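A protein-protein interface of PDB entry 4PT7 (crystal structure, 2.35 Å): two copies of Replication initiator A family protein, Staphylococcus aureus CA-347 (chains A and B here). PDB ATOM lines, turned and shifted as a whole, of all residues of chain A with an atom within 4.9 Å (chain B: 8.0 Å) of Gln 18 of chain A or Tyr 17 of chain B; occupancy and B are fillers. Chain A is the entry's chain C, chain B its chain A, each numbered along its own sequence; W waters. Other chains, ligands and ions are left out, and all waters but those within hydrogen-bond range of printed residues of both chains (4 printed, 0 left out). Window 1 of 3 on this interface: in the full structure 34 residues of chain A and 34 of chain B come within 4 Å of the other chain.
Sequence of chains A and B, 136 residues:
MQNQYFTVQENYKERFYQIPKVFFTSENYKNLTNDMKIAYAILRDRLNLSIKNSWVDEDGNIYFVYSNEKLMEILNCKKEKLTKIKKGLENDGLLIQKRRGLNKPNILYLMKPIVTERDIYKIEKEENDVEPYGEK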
ATOM      1  N   PHE A  16      -8.271 -20.116 -14.648  1.00  0.00           N
ATOM      2  CA  PHE A  16      -7.377 -20.815 -15.558  1.00  0.00           C
ATOM      3  C   PHE A  16      -6.086 -20.072 -15.876  1.00  0.00           C
ATOM      4  O   PHE A  16      -5.890 -18.921 -15.488  1.00  0.00           O
ATOM      5  CB  PHE A  16      -8.074 -21.107 -16.911  1.00  0.00           C
ATOM      6  CG  PHE A  16      -9.581 -21.242 -16.835  1.00  0.00           C
ATOM      7  CD1 PHE A  16     -10.380 -20.122 -16.634  1.00  0.00           C
ATOM      8  CD2 PHE A  16     -10.202 -22.485 -16.992  1.00  0.00           C
ATOM      9  CE1 PHE A  16     -11.779 -20.228 -16.588  1.00  0.00           C
ATOM     10  CE2 PHE A  16     -11.603 -22.604 -16.946  1.00  0.00           C
ATOM     11  CZ  PHE A  16     -12.390 -21.468 -16.744  1.00  0.00           C
ATOM     12  N   TYR A  17      -5.205 -20.769 -16.581  1.00  0.00           N
ATOM     13  CA  TYR A  17      -3.967 -20.208 -17.079  1.00  0.00           C
ATOM     14  C   TYR A  17      -4.316 -20.115 -18.551  1.00  0.00           C
ATOM     15  O   TYR A  17      -4.918 -21.035 -19.105  1.00  0.00           O
ATOM     16  CB  TYR A  17      -2.795 -21.165 -16.863  1.00  0.00           C
ATOM     17  CG  TYR A  17      -2.334 -21.198 -15.429  1.00  0.00           C
ATOM     18  CD1 TYR A  17      -2.209 -22.409 -14.752  1.00  0.00           C
ATOM     19  CD2 TYR A  17      -2.048 -20.013 -14.736  1.00  0.00           C
ATOM     20  CE1 TYR A  17      -1.812 -22.443 -13.414  1.00  0.00           C
ATOM     21  CE2 TYR A  17      -1.656 -20.036 -13.408  1.00  0.00           C
ATOM     22  CZ  TYR A  17      -1.538 -21.253 -12.752  1.00  0.00           C
ATOM     23  OH  TYR A  17      -1.137 -21.282 -11.441  1.00  0.00           O
ATOM     24  N   GLN A  18      -3.965 -18.995 -19.171  1.00  0.00           N
ATOM     25  CA  GLN A  18      -4.291 -18.755 -20.574  1.00  0.00           C
ATOM     26  C   GLN A  18      -3.112 -18.837 -21.525  1.00  0.00           C
ATOM     27  O   GLN A  18      -2.144 -18.077 -21.398  1.00  0.00           O
ATOM     28  CB  GLN A  18      -4.946 -17.368 -20.726  1.00  0.00           C
ATOM     29  CG  GLN A  18      -6.255 -17.211 -19.991  1.00  0.00           C
ATOM     30  CD  GLN A  18      -6.763 -15.770 -19.989  1.00  0.00           C
ATOM     31  OE1 GLN A  18      -7.945 -15.518 -20.233  1.00  0.00           O
ATOM     32  NE2 GLN A  18      -5.872 -14.821 -19.703  1.00  0.00           N
ATOM     33  N   ILE A  19      -3.210 -19.727 -22.506  1.00  0.00           N
ATOM     34  CA  ILE A  19      -2.150 -19.867 -23.490  1.00  0.00           C
ATOM     35  C   ILE A  19      -2.622 -19.281 -24.811  1.00  0.00           C
ATOM     36  O   ILE A  19      -3.697 -19.623 -25.299  1.00  0.00           O
ATOM     37  CB  ILE A  19      -1.776 -21.347 -23.724  1.00  0.00           C
ATOM     38  CG1 ILE A  19      -1.397 -22.013 -22.399  1.00  0.00           C
ATOM     39  CG2 ILE A  19      -0.595 -21.434 -24.697  1.00  0.00           C
ATOM     40  CD1 ILE A  19      -1.195 -23.513 -22.508  1.00  0.00           C
ATOM     41  N   PRO A  20      -1.832 -18.368 -25.394  1.00  0.00           N
ATOM     42  CA  PRO A  20      -2.194 -17.750 -26.672  1.00  0.00           C
ATOM     43  C   PRO A  20      -2.388 -18.814 -27.752  1.00  0.00           C
ATOM     44  O   PRO A  20      -1.536 -19.690 -27.928  1.00  0.00           O
ATOM     45  CB  PRO A  20      -0.996 -16.851 -26.970  1.00  0.00           C
ATOM     46  CG  PRO A  20      -0.556 -16.430 -25.612  1.00  0.00           C
ATOM     47  CD  PRO A  20      -0.647 -17.713 -24.812  1.00  0.00           C
ATOM     48  N   LYS A  21      -3.504 -18.732 -28.473  1.00  0.00           N
ATOM     49  CA  LYS A  21      -3.807 -19.681 -29.540  1.00  0.00           C
ATOM     50  C   LYS A  21      -2.748 -19.637 -30.635  1.00  0.00           C
ATOM     51  O   LYS A  21      -2.476 -20.643 -31.295  1.00  0.00           O
ATOM     52  CB  LYS A  21      -5.184 -19.385 -30.152  1.00  0.00           C
ATOM     53  CG  LYS A  21      -6.372 -19.747 -29.257  1.00  0.00           C
ATOM     54  CD  LYS A  21      -7.672 -19.808 -30.075  1.00  0.00           C
ATOM     55  CE  LYS A  21      -8.849 -20.177 -29.201  1.00  0.00           C
ATOM     56  NZ  LYS A  21     -10.128 -20.266 -29.982  1.00  0.00           N
ATOM     57  N   PHE A  24      -0.233 -22.292 -31.191  1.00  0.00           N
ATOM     58  CA  PHE A  24      -0.573 -23.572 -31.799  1.00  0.00           C
ATOM     59  C   PHE A  24      -0.908 -23.450 -33.282  1.00  0.00           C
ATOM     60  O   PHE A  24      -1.200 -24.442 -33.940  1.00  0.00           O
ATOM     61  CB  PHE A  24      -1.755 -24.221 -31.073  1.00  0.00           C
ATOM     62  CG  PHE A  24      -1.541 -24.405 -29.599  1.00  0.00           C
ATOM     63  CD1 PHE A  24      -1.876 -23.396 -28.703  1.00  0.00           C
ATOM     64  CD2 PHE A  24      -1.028 -25.599 -29.099  1.00  0.00           C
ATOM     65  CE1 PHE A  24      -1.708 -23.575 -27.323  1.00  0.00           C
ATOM     66  CE2 PHE A  24      -0.854 -25.789 -27.726  1.00  0.00           C
ATOM     67  CZ  PHE A  24      -1.197 -24.774 -26.837  1.00  0.00           C
ATOM     68  N   ALA A  41       2.034 -19.140 -19.888  1.00  0.00           N
ATOM     69  CA  ALA A  41       0.703 -18.846 -19.372  1.00  0.00           C
ATOM     70  C   ALA A  41       0.711 -18.603 -17.865  1.00  0.00           C
ATOM     71  O   ALA A  41      -0.030 -17.763 -17.363  1.00  0.00           O
ATOM     72  CB  ALA A  41      -0.257 -19.973 -19.730  1.00  0.00           C
ATOM     73  N   ARG A  44       2.157 -15.233 -17.198  1.00  0.00           N
ATOM     74  CA  ARG A  44       1.191 -14.231 -17.638  1.00  0.00           C
ATOM     75  C   ARG A  44       0.241 -13.920 -16.489  1.00  0.00           C
ATOM     76  O   ARG A  44      -0.070 -12.760 -16.215  1.00  0.00           O
ATOM     77  CB  ARG A  44       0.400 -14.753 -18.846  1.00  0.00           C
ATOM     78  CG  ARG A  44      -0.735 -13.849 -19.278  1.00  0.00           C
ATOM     79  CD  ARG A  44      -1.509 -14.441 -20.442  1.00  0.00           C
ATOM     80  NE  ARG A  44      -1.591 -13.443 -21.494  1.00  0.00           N
ATOM     81  CZ  ARG A  44      -2.508 -12.489 -21.555  1.00  0.00           C
ATOM     82  NH1 ARG A  44      -2.469 -11.614 -22.546  1.00  0.00           N
ATOM     83  NH2 ARG A  44      -3.488 -12.442 -20.666  1.00  0.00           N
ATOM     84  N   GLU A 126     -10.271 -22.048 -37.726  1.00  0.00           N
ATOM     85  CA  GLU A 126     -10.458 -23.071 -36.705  1.00  0.00           C
ATOM     86  C   GLU A 126     -11.680 -22.833 -35.829  1.00  0.00           C
ATOM     87  O   GLU A 126     -12.410 -23.767 -35.512  1.00  0.00           O
ATOM     88  CB  GLU A 126      -9.227 -23.186 -35.802  1.00  0.00           C
ATOM     89  CG  GLU A 126      -8.004 -23.788 -36.466  1.00  0.00           C
ATOM     90  CD  GLU A 126      -6.928 -24.149 -35.449  1.00  0.00           C
ATOM     91  OE1 GLU A 126      -7.213 -24.973 -34.548  1.00  0.00           O
ATOM     92  OE2 GLU A 126      -5.804 -23.607 -35.543  1.00  0.00           O
ATOM     93  N   GLU B  14      -5.106 -11.728 -28.295  1.00  0.00           N
ATOM     94  CA  GLU B  14      -5.778 -11.983 -27.024  1.00  0.00           C
ATOM     95  C   GLU B  14      -6.789 -13.137 -27.048  1.00  0.00           C
ATOM     96  O   GLU B  14      -7.795 -13.116 -26.346  1.00  0.00           O
ATOM     97  CB  GLU B  14      -6.462 -10.705 -26.524  1.00  0.00           C
ATOM     98  CG  GLU B  14      -5.490  -9.623 -26.005  1.00  0.00           C
ATOM     99  CD  GLU B  14      -4.733 -10.053 -24.743  1.00  0.00           C
ATOM    100  OE1 GLU B  14      -5.388 -10.356 -23.717  1.00  0.00           O
ATOM    101  OE2 GLU B  14      -3.479 -10.091 -24.782  1.00  0.00           O
ATOM    102  N   ARG B  15      -6.503 -14.147 -27.859  1.00  0.00           N
ATOM    103  CA  ARG B  15      -7.340 -15.345 -27.945  1.00  0.00           C
ATOM    104  C   ARG B  15      -6.530 -16.481 -27.327  1.00  0.00           C
ATOM    105  O   ARG B  15      -5.369 -16.698 -27.707  1.00  0.00           O
ATOM    106  CB  ARG B  15      -7.664 -15.677 -29.398  1.00  0.00           C
ATOM    107  CG  ARG B  15      -8.846 -14.900 -29.970  1.00  0.00           C
ATOM    108  CD  ARG B  15      -9.245 -15.511 -31.293  1.00  0.00           C
ATOM    109  NE  ARG B  15     -10.462 -14.949 -31.866  1.00  0.00           N
ATOM    110  CZ  ARG B  15     -10.572 -13.707 -32.316  1.00  0.00           C
ATOM    111  NH1 ARG B  15      -9.536 -12.886 -32.253  1.00  0.00           N
ATOM    112  NH2 ARG B  15     -11.707 -13.299 -32.858  1.00  0.00           N
ATOM    113  N   PHE B  16      -7.112 -17.206 -26.377  1.00  0.00           N
ATOM    114  CA  PHE B  16      -6.353 -18.272 -25.743  1.00  0.00           C
ATOM    115  C   PHE B  16      -7.135 -19.546 -25.459  1.00  0.00           C
ATOM    116  O   PHE B  16      -8.360 -19.616 -25.618  1.00  0.00           O
ATOM    117  CB  PHE B  16      -5.743 -17.804 -24.398  1.00  0.00           C
ATOM    118  CG  PHE B  16      -5.554 -16.315 -24.263  1.00  0.00           C
ATOM    119  CD1 PHE B  16      -6.652 -15.476 -24.083  1.00  0.00           C
ATOM    120  CD2 PHE B  16      -4.272 -15.753 -24.245  1.00  0.00           C
ATOM    121  CE1 PHE B  16      -6.481 -14.094 -23.883  1.00  0.00           C
ATOM    122  CE2 PHE B  16      -4.097 -14.366 -24.044  1.00  0.00           C
ATOM    123  CZ  PHE B  16      -5.204 -13.544 -23.863  1.00  0.00           C
ATOM    124  N   TYR B  17      -6.381 -20.566 -25.053  1.00  0.00           N
ATOM    125  CA  TYR B  17      -6.934 -21.839 -24.627  1.00  0.00           C
ATOM    126  C   TYR B  17      -6.790 -21.728 -23.121  1.00  0.00           C
ATOM    127  O   TYR B  17      -5.781 -21.218 -22.617  1.00  0.00           O
ATOM    128  CB  TYR B  17      -6.126 -23.008 -25.173  1.00  0.00           C
ATOM    129  CG  TYR B  17      -6.365 -23.221 -26.643  1.00  0.00           C
ATOM    130  CD1 TYR B  17      -5.311 -23.167 -27.556  1.00  0.00           C
ATOM    131  CD2 TYR B  17      -7.655 -23.452 -27.129  1.00  0.00           C
ATOM    132  CE1 TYR B  17      -5.531 -23.335 -28.917  1.00  0.00           C
ATOM    133  CE2 TYR B  17      -7.891 -23.625 -28.500  1.00  0.00           C
ATOM    134  CZ  TYR B  17      -6.821 -23.565 -29.382  1.00  0.00           C
ATOM    135  OH  TYR B  17      -7.032 -23.744 -30.725  1.00  0.00           O
ATOM    136  N   GLN B  18      -7.817 -22.165 -22.409  1.00  0.00           N
ATOM    137  CA  GLN B  18      -7.834 -22.055 -20.965  1.00  0.00           C
ATOM    138  C   GLN B  18      -7.677 -23.373 -20.244  1.00  0.00           C
ATOM    139  O   GLN B  18      -8.479 -24.286 -20.426  1.00  0.00           O
ATOM    140  CB  GLN B  18      -9.155 -21.417 -20.510  1.00  0.00           C
ATOM    141  CG  GLN B  18      -9.484 -20.107 -21.187  1.00  0.00           C
ATOM    142  CD  GLN B  18     -10.855 -19.566 -20.767  1.00  0.00           C
ATOM    143  OE1 GLN B  18     -11.889 -20.202 -20.999  1.00  0.00           O
ATOM    144  NE2 GLN B  18     -10.861 -18.398 -20.139  1.00  0.00           N
ATOM    145  N   ILE B  19      -6.668 -23.456 -19.387  1.00  0.00           N
ATOM    146  CA  ILE B  19      -6.462 -24.669 -18.623  1.00  0.00           C
ATOM    147  C   ILE B  19      -6.830 -24.391 -17.178  1.00  0.00           C
ATOM    148  O   ILE B  19      -6.350 -23.425 -16.591  1.00  0.00           O
ATOM    149  CB  ILE B  19      -5.010 -25.120 -18.657  1.00  0.00           C
ATOM    150  CG1 ILE B  19      -4.543 -25.281 -20.107  1.00  0.00           C
ATOM    151  CG2 ILE B  19      -4.872 -26.424 -17.889  1.00  0.00           C
ATOM    152  CD1 ILE B  19      -3.096 -25.718 -20.225  1.00  0.00           C
ATOM    153  N   PRO B  20      -7.690 -25.229 -16.585  1.00  0.00           N
ATOM    154  CA  PRO B  20      -8.078 -25.014 -15.186  1.00  0.00           C
ATOM    155  C   PRO B  20      -6.838 -25.030 -14.288  1.00  0.00           C
ATOM    156  O   PRO B  20      -5.982 -25.912 -14.419  1.00  0.00           O
ATOM    157  CB  PRO B  20      -9.013 -26.190 -14.904  1.00  0.00           C
ATOM    158  CG  PRO B  20      -9.620 -26.464 -16.250  1.00  0.00           C
ATOM    159  CD  PRO B  20      -8.443 -26.344 -17.185  1.00  0.00           C
ATOM    160  N   LYS B  21      -6.750 -24.065 -13.374  1.00  0.00           N
ATOM    161  CA  LYS B  21      -5.609 -23.979 -12.466  1.00  0.00           C
ATOM    162  C   LYS B  21      -5.540 -25.204 -11.570  1.00  0.00           C
ATOM    163  O   LYS B  21      -4.458 -25.651 -11.191  1.00  0.00           O
ATOM    164  CB  LYS B  21      -5.707 -22.725 -11.598  1.00  0.00           C
ATOM    165  CG  LYS B  21      -5.475 -21.430 -12.350  1.00  0.00           C
ATOM    166  CD  LYS B  21      -5.242 -20.281 -11.374  1.00  0.00           C
ATOM    167  CE  LYS B  21      -4.861 -18.998 -12.092  1.00  0.00           C
ATOM    168  NZ  LYS B  21      -4.446 -17.966 -11.104  1.00  0.00           N
ATOM    169  N   LYS B  37      -3.711 -31.832 -20.357  1.00  0.00           N
ATOM    170  CA  LYS B  37      -4.173 -30.531 -19.885  1.00  0.00           C
ATOM    171  C   LYS B  37      -4.468 -29.625 -21.074  1.00  0.00           C
ATOM    172  O   LYS B  37      -5.527 -28.995 -21.141  1.00  0.00           O
ATOM    173  CB  LYS B  37      -3.113 -29.902 -18.983  1.00  0.00           C
ATOM    174  CG  LYS B  37      -2.836 -30.726 -17.727  1.00  0.00           C
ATOM    175  CD  LYS B  37      -1.767 -30.105 -16.844  1.00  0.00           C
ATOM    176  CE  LYS B  37      -1.446 -31.035 -15.665  1.00  0.00           C
ATOM    177  NZ  LYS B  37      -0.391 -30.505 -14.753  1.00  0.00           N
ATOM    178  N   ILE B  38      -3.531 -29.583 -22.016  1.00  0.00           N
ATOM    179  CA  ILE B  38      -3.687 -28.774 -23.212  1.00  0.00           C
ATOM    180  C   ILE B  38      -4.839 -29.288 -24.084  1.00  0.00           C
ATOM    181  O   ILE B  38      -5.605 -28.498 -24.625  1.00  0.00           O
ATOM    182  CB  ILE B  38      -2.375 -28.742 -24.027  1.00  0.00           C
ATOM    183  CG1 ILE B  38      -1.299 -28.006 -23.218  1.00  0.00           C
ATOM    184  CG2 ILE B  38      -2.594 -28.078 -25.377  1.00  0.00           C
ATOM    185  CD1 ILE B  38       0.031 -27.865 -23.937  1.00  0.00           C
ATOM    186  N   ALA B  39      -4.976 -30.603 -24.205  1.00  0.00           N
ATOM    187  CA  ALA B  39      -6.053 -31.163 -25.015  1.00  0.00           C
ATOM    188  C   ALA B  39      -7.391 -30.763 -24.407  1.00  0.00           C
ATOM    189  O   ALA B  39      -8.319 -30.384 -25.117  1.00  0.00           O
ATOM    190  CB  ALA B  39      -5.944 -32.683 -25.079  1.00  0.00           C
ATOM    191  N   TYR B  40      -7.485 -30.868 -23.086  1.00  0.00           N
ATOM    192  CA  TYR B  40      -8.699 -30.501 -22.376  1.00  0.00           C
ATOM    193  C   TYR B  40      -9.079 -29.045 -22.699  1.00  0.00           C
ATOM    194  O   TYR B  40     -10.229 -28.759 -23.005  1.00  0.00           O
ATOM    195  CB  TYR B  40      -8.491 -30.661 -20.870  1.00  0.00           C
ATOM    196  CG  TYR B  40      -9.705 -30.308 -20.041  1.00  0.00           C
ATOM    197  CD1 TYR B  40     -10.646 -31.279 -19.696  1.00  0.00           C
ATOM    198  CD2 TYR B  40      -9.931 -28.985 -19.630  1.00  0.00           C
ATOM    199  CE1 TYR B  40     -11.797 -30.941 -18.961  1.00  0.00           C
ATOM    200  CE2 TYR B  40     -11.059 -28.640 -18.908  1.00  0.00           C
ATOM    201  CZ  TYR B  40     -11.991 -29.615 -18.576  1.00  0.00           C
ATOM    202  OH  TYR B  40     -13.116 -29.259 -17.870  1.00  0.00           O
ATOM    203  N   ALA B  41      -8.105 -28.141 -22.648  1.00  0.00           N
ATOM    204  CA  ALA B  41      -8.340 -26.719 -22.916  1.00  0.00           C
ATOM    205  C   ALA B  41      -8.824 -26.482 -24.335  1.00  0.00           C
ATOM    206  O   ALA B  41      -9.691 -25.641 -24.572  1.00  0.00           O
ATOM    207  CB  ALA B  41      -7.055 -25.914 -22.666  1.00  0.00           C
ATOM    208  N   ILE B  42      -8.246 -27.211 -25.279  1.00  0.00           N
ATOM    209  CA  ILE B  42      -8.638 -27.069 -26.669  1.00  0.00           C
ATOM    210  C   ILE B  42     -10.072 -27.559 -26.850  1.00  0.00           C
ATOM    211  O   ILE B  42     -10.854 -26.945 -27.576  1.00  0.00           O
ATOM    212  CB  ILE B  42      -7.686 -27.849 -27.603  1.00  0.00           C
ATOM    213  CG1 ILE B  42      -6.274 -27.246 -27.513  1.00  0.00           C
ATOM    214  CG2 ILE B  42      -8.217 -27.819 -29.037  1.00  0.00           C
ATOM    215  CD1 ILE B  42      -5.220 -27.944 -28.370  1.00  0.00           C
ATOM    216  N   LEU B  43     -10.429 -28.651 -26.176  1.00  0.00           N
ATOM    217  CA  LEU B  43     -11.782 -29.184 -26.284  1.00  0.00           C
ATOM    218  C   LEU B  43     -12.787 -28.251 -25.587  1.00  0.00           C
ATOM    219  O   LEU B  43     -13.927 -28.122 -26.035  1.00  0.00           O
ATOM    220  CB  LEU B  43     -11.857 -30.606 -25.703  1.00  0.00           C
ATOM    221  CG  LEU B  43     -11.082 -31.701 -26.464  1.00  0.00           C
ATOM    222  CD1 LEU B  43     -11.289 -33.073 -25.828  1.00  0.00           C
ATOM    223  CD2 LEU B  43     -11.541 -31.736 -27.908  1.00  0.00           C
ATOM    224  N   ARG B  44     -12.360 -27.600 -24.500  1.00  0.00           N
ATOM    225  CA  ARG B  44     -13.230 -26.662 -23.789  1.00  0.00           C
ATOM    226  C   ARG B  44     -13.589 -25.540 -24.769  1.00  0.00           C
ATOM    227  O   ARG B  44     -14.722 -25.061 -24.791  1.00  0.00           O
ATOM    228  CB  ARG B  44     -12.517 -26.092 -22.552  1.00  0.00           C
ATOM    229  CG  ARG B  44     -13.103 -24.784 -22.053  1.00  0.00           C
ATOM    230  CD  ARG B  44     -12.314 -24.166 -20.907  1.00  0.00           C
ATOM    231  NE  ARG B  44     -13.119 -24.270 -19.705  1.00  0.00           N
ATOM    232  CZ  ARG B  44     -13.956 -23.337 -19.275  1.00  0.00           C
ATOM    233  NH1 ARG B  44     -14.655 -23.558 -18.182  1.00  0.00           N
ATOM    234  NH2 ARG B  44     -14.051 -22.170 -19.892  1.00  0.00           N
ATOM    235  N   ASP B  45     -12.620 -25.140 -25.589  1.00  0.00           N
ATOM    236  CA  ASP B  45     -12.843 -24.095 -26.581  1.00  0.00           C
ATOM    237  C   ASP B  45     -13.789 -24.569 -27.689  1.00  0.00           C
ATOM    238  O   ASP B  45     -14.594 -23.782 -28.193  1.00  0.00           O
ATOM    239  CB  ASP B  45     -11.513 -23.652 -27.195  1.00  0.00           C
ATOM    240  CG  ASP B  45     -11.677 -22.552 -28.237  1.00  0.00           C
ATOM    241  OD1 ASP B  45     -11.835 -21.374 -27.853  1.00  0.00           O
ATOM    242  OD2 ASP B  45     -11.649 -22.868 -29.446  1.00  0.00           O
ATOM    243  N   ARG B  46     -13.694 -25.848 -28.064  1.00  0.00           N
ATOM    244  CA  ARG B  46     -14.538 -26.402 -29.129  1.00  0.00           C
ATOM    245  C   ARG B  46     -16.016 -26.445 -28.741  1.00  0.00           C
ATOM    246  O   ARG B  46     -16.879 -26.591 -29.600  1.00  0.00           O
ATOM    247  CB  ARG B  46     -14.110 -27.837 -29.507  1.00  0.00           C
ATOM    248  CG  ARG B  46     -12.809 -27.967 -30.252  1.00  0.00           C
ATOM    249  CD  ARG B  46     -12.787 -27.260 -31.607  1.00  0.00           C
ATOM    250  NE  ARG B  46     -13.499 -27.971 -32.663  1.00  0.00           N
ATOM    251  CZ  ARG B  46     -13.117 -27.958 -33.937  1.00  0.00           C
ATOM    252  NH1 ARG B  46     -12.031 -27.284 -34.299  1.00  0.00           N
ATOM    253  NH2 ARG B  46     -13.825 -28.587 -34.858  1.00  0.00           N
ATOM    254  N   ILE B  74      -8.011 -31.879 -34.723  1.00  0.00           N
ATOM    255  CA  ILE B  74      -8.344 -30.818 -33.773  1.00  0.00           C
ATOM    256  C   ILE B  74      -7.214 -30.639 -32.759  1.00  0.00           C
ATOM    257  O   ILE B  74      -6.684 -29.537 -32.590  1.00  0.00           O
ATOM    258  CB  ILE B  74      -9.674 -31.145 -33.030  1.00  0.00           C
ATOM    259  CG1 ILE B  74     -10.862 -30.939 -33.984  1.00  0.00           C
ATOM    260  CG2 ILE B  74      -9.807 -30.285 -31.770  1.00  0.00           C
ATOM    261  CD1 ILE B  74     -12.215 -31.402 -33.443  1.00  0.00           C
HETATM  262  O   HOH W   1      -9.376 -22.531 -31.884  1.00  0.00           O
HETATM  263  O   HOH W   2      -3.577 -15.997 -29.884  1.00  0.00           O
HETATM  264  O   HOH W   3      -7.808 -27.112 -33.196  1.00  0.00           O
HETATM  265  O   HOH W   4      -1.892 -19.100  -9.859  1.00  0.00           O
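The side-chain carboxylate (OE2) of Glu 14 of chain B is in salt-bridge range of the guanidinium group (NH1) of Arg 44 of chain A.
The backbone carbonyl oxygen (O) of Arg 15 of chain B lies within hydrogen-bond range of the backbone NH (N) of Lys 21 of chain A.
The backbone carbonyl oxygen (O) of Ile 19 of chain A lies within hydrogen-bond range of the backbone NH (N) of Tyr 17 of chain B (2.9 Å).
O of Ile 19 of chain B lies within hydrogen-bond range of N of Tyr 17 of chain A (2.9 Å).
The side-chain amino group (NZ) of Lys 21 of chain A lies within salt-bridge range of the side-chain carboxylate (OD1) of Asp 45 of chain B (2.9 Å).
NH2 of Arg 44 of chain B is in hydrogen-bond range of OE1 of Gln 18 of chain B (3.1 Å).
Phe 16 of chain A touches Pro 20 of chain B (CD2 to N, 3.7 Å).
CZ of Arg 44 of chain B touches CE2 of Phe 16 of chain A, at 3.4 Å.
Tyr 17 of chain A touches Tyr 17 of chain B.
Ile 19 of chain A touches Phe 16 of chain B.
CD1 of Ile 19 of chain A touches CD1 of Ile 19 of chain B, at 3.7 Å.
Tyr 17 of chain B touches Lys 21 of chain A (CE2 to CE, 3.6 Å).
Tyr 17 of chain B touches Phe 24 of chain A.
Ile 38 of chain B touches Phe 24 of chain A (CG2 to CE2, 3.7 Å).
Arg 44 of chain A touches Phe 16 of chain B (CZ to CE2, 3.5 Å).
NH1 of Arg 46 of chain B touches O of Glu 126 of chain A, at 3.7 Å.
Gln 18 of chain A touches just these residues of chain B: Phe 16 and Tyr 17.
Printed residues of chain A within 4 Å of Tyr 17 of chain B: Tyr 17 (3.6 Å), Gln 18 (3.5 Å), Ile 19 (2.9 Å), Lys 21 (3.6 Å) and Phe 24 (3.6 Å).
Of the printed residues of chain A, Gln 18 of chain B touches Phe 16 and Tyr 17.
Printed residues of chain A within 4 Å of Pro 20 of chain B: Phe 16 (3.7 Å).
Of the printed residues of chain B, Ile 19 of chain A touches Phe 16 (2.9 Å), Tyr 17 (2.9 Å) and Ile 19 (3.7 Å).
Printed residues of chain A within 4 Å of Arg 46 of chain B: Glu 126.
Ile 42 of chain B touches none of the printed residues of chain A.
The nearest residue of chain B that does not touch Gln 18 of chain A is Gln 18 of chain B (4.1 Å).
The nearest printed residue of chain A that does not touch Tyr 17 of chain B is Glu 126 of chain A (4.02 Å).
Hydrophobic or aromatic side chains of chain A that line the printed part of chain B: Phe 16, Tyr 17, Ile 19 and Phe 24.
Of the 19 printed residues of chain B, 12 touch a printed residue of chain A.
Among the printed residues, 25 pairs touch across the chains.
Among the printed residues, Asp or Glu carboxylates within 4 Å of a Lys or Arg side-chain nitrogen of the other chain: Lys 21 of chain A with Asp 45 of chain B and Arg 44 of chain A with Glu 14 of chain B.
Phe 16 of chain A touches Gln 18 of chain B, and with the chains exchanged Gln 18 of chain A touches Phe 16 of chain B.
Phe 16 of chain A touches Pro 20 of chain B, and with the chains exchanged Pro 20 of chain A touches Phe 16 of chain B.
Phe 16 of chain A touches Lys 21 of chain B, and with the chains exchanged Lys 21 of chain A touches Phe 16 of chain B.
Tyr 17 of chain A touches Ile 19 of chain B, and with the chains exchanged Ile 19 of chain A touches Tyr 17 of chain B.
Positions printed for both chains: 16, 17, 18, 19, 20, 21, 41 and 44.
Of the 25 pairs that touch across the chains among the printed residues, 18 have their exchanged pair printed and touching as well.
Water W3 bridges OE1 of Glu 126 of chain A (2.6 Å) and O of Ile 74 of chain B (2.7 Å).
Water W4 bridges the side-chain hydroxyl of Tyr 17 of chain A (2.8 Å) and the side-chain amino group of Lys 21 of chain B (3.1 Å).
Water W1 lies within hydrogen-bond range of the side-chain hydroxyl of Tyr 17 of chain B (2.9 Å), the side-chain amino group of Lys 21 of chain A (3.1 Å) and the side-chain carboxylate of Asp 45 of chain B (3.4 Å).
Water W2 lies within hydrogen-bond range of O of Arg 15 of chain B (2.9 Å) and N of Lys 21 of chain A (3.1 Å).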
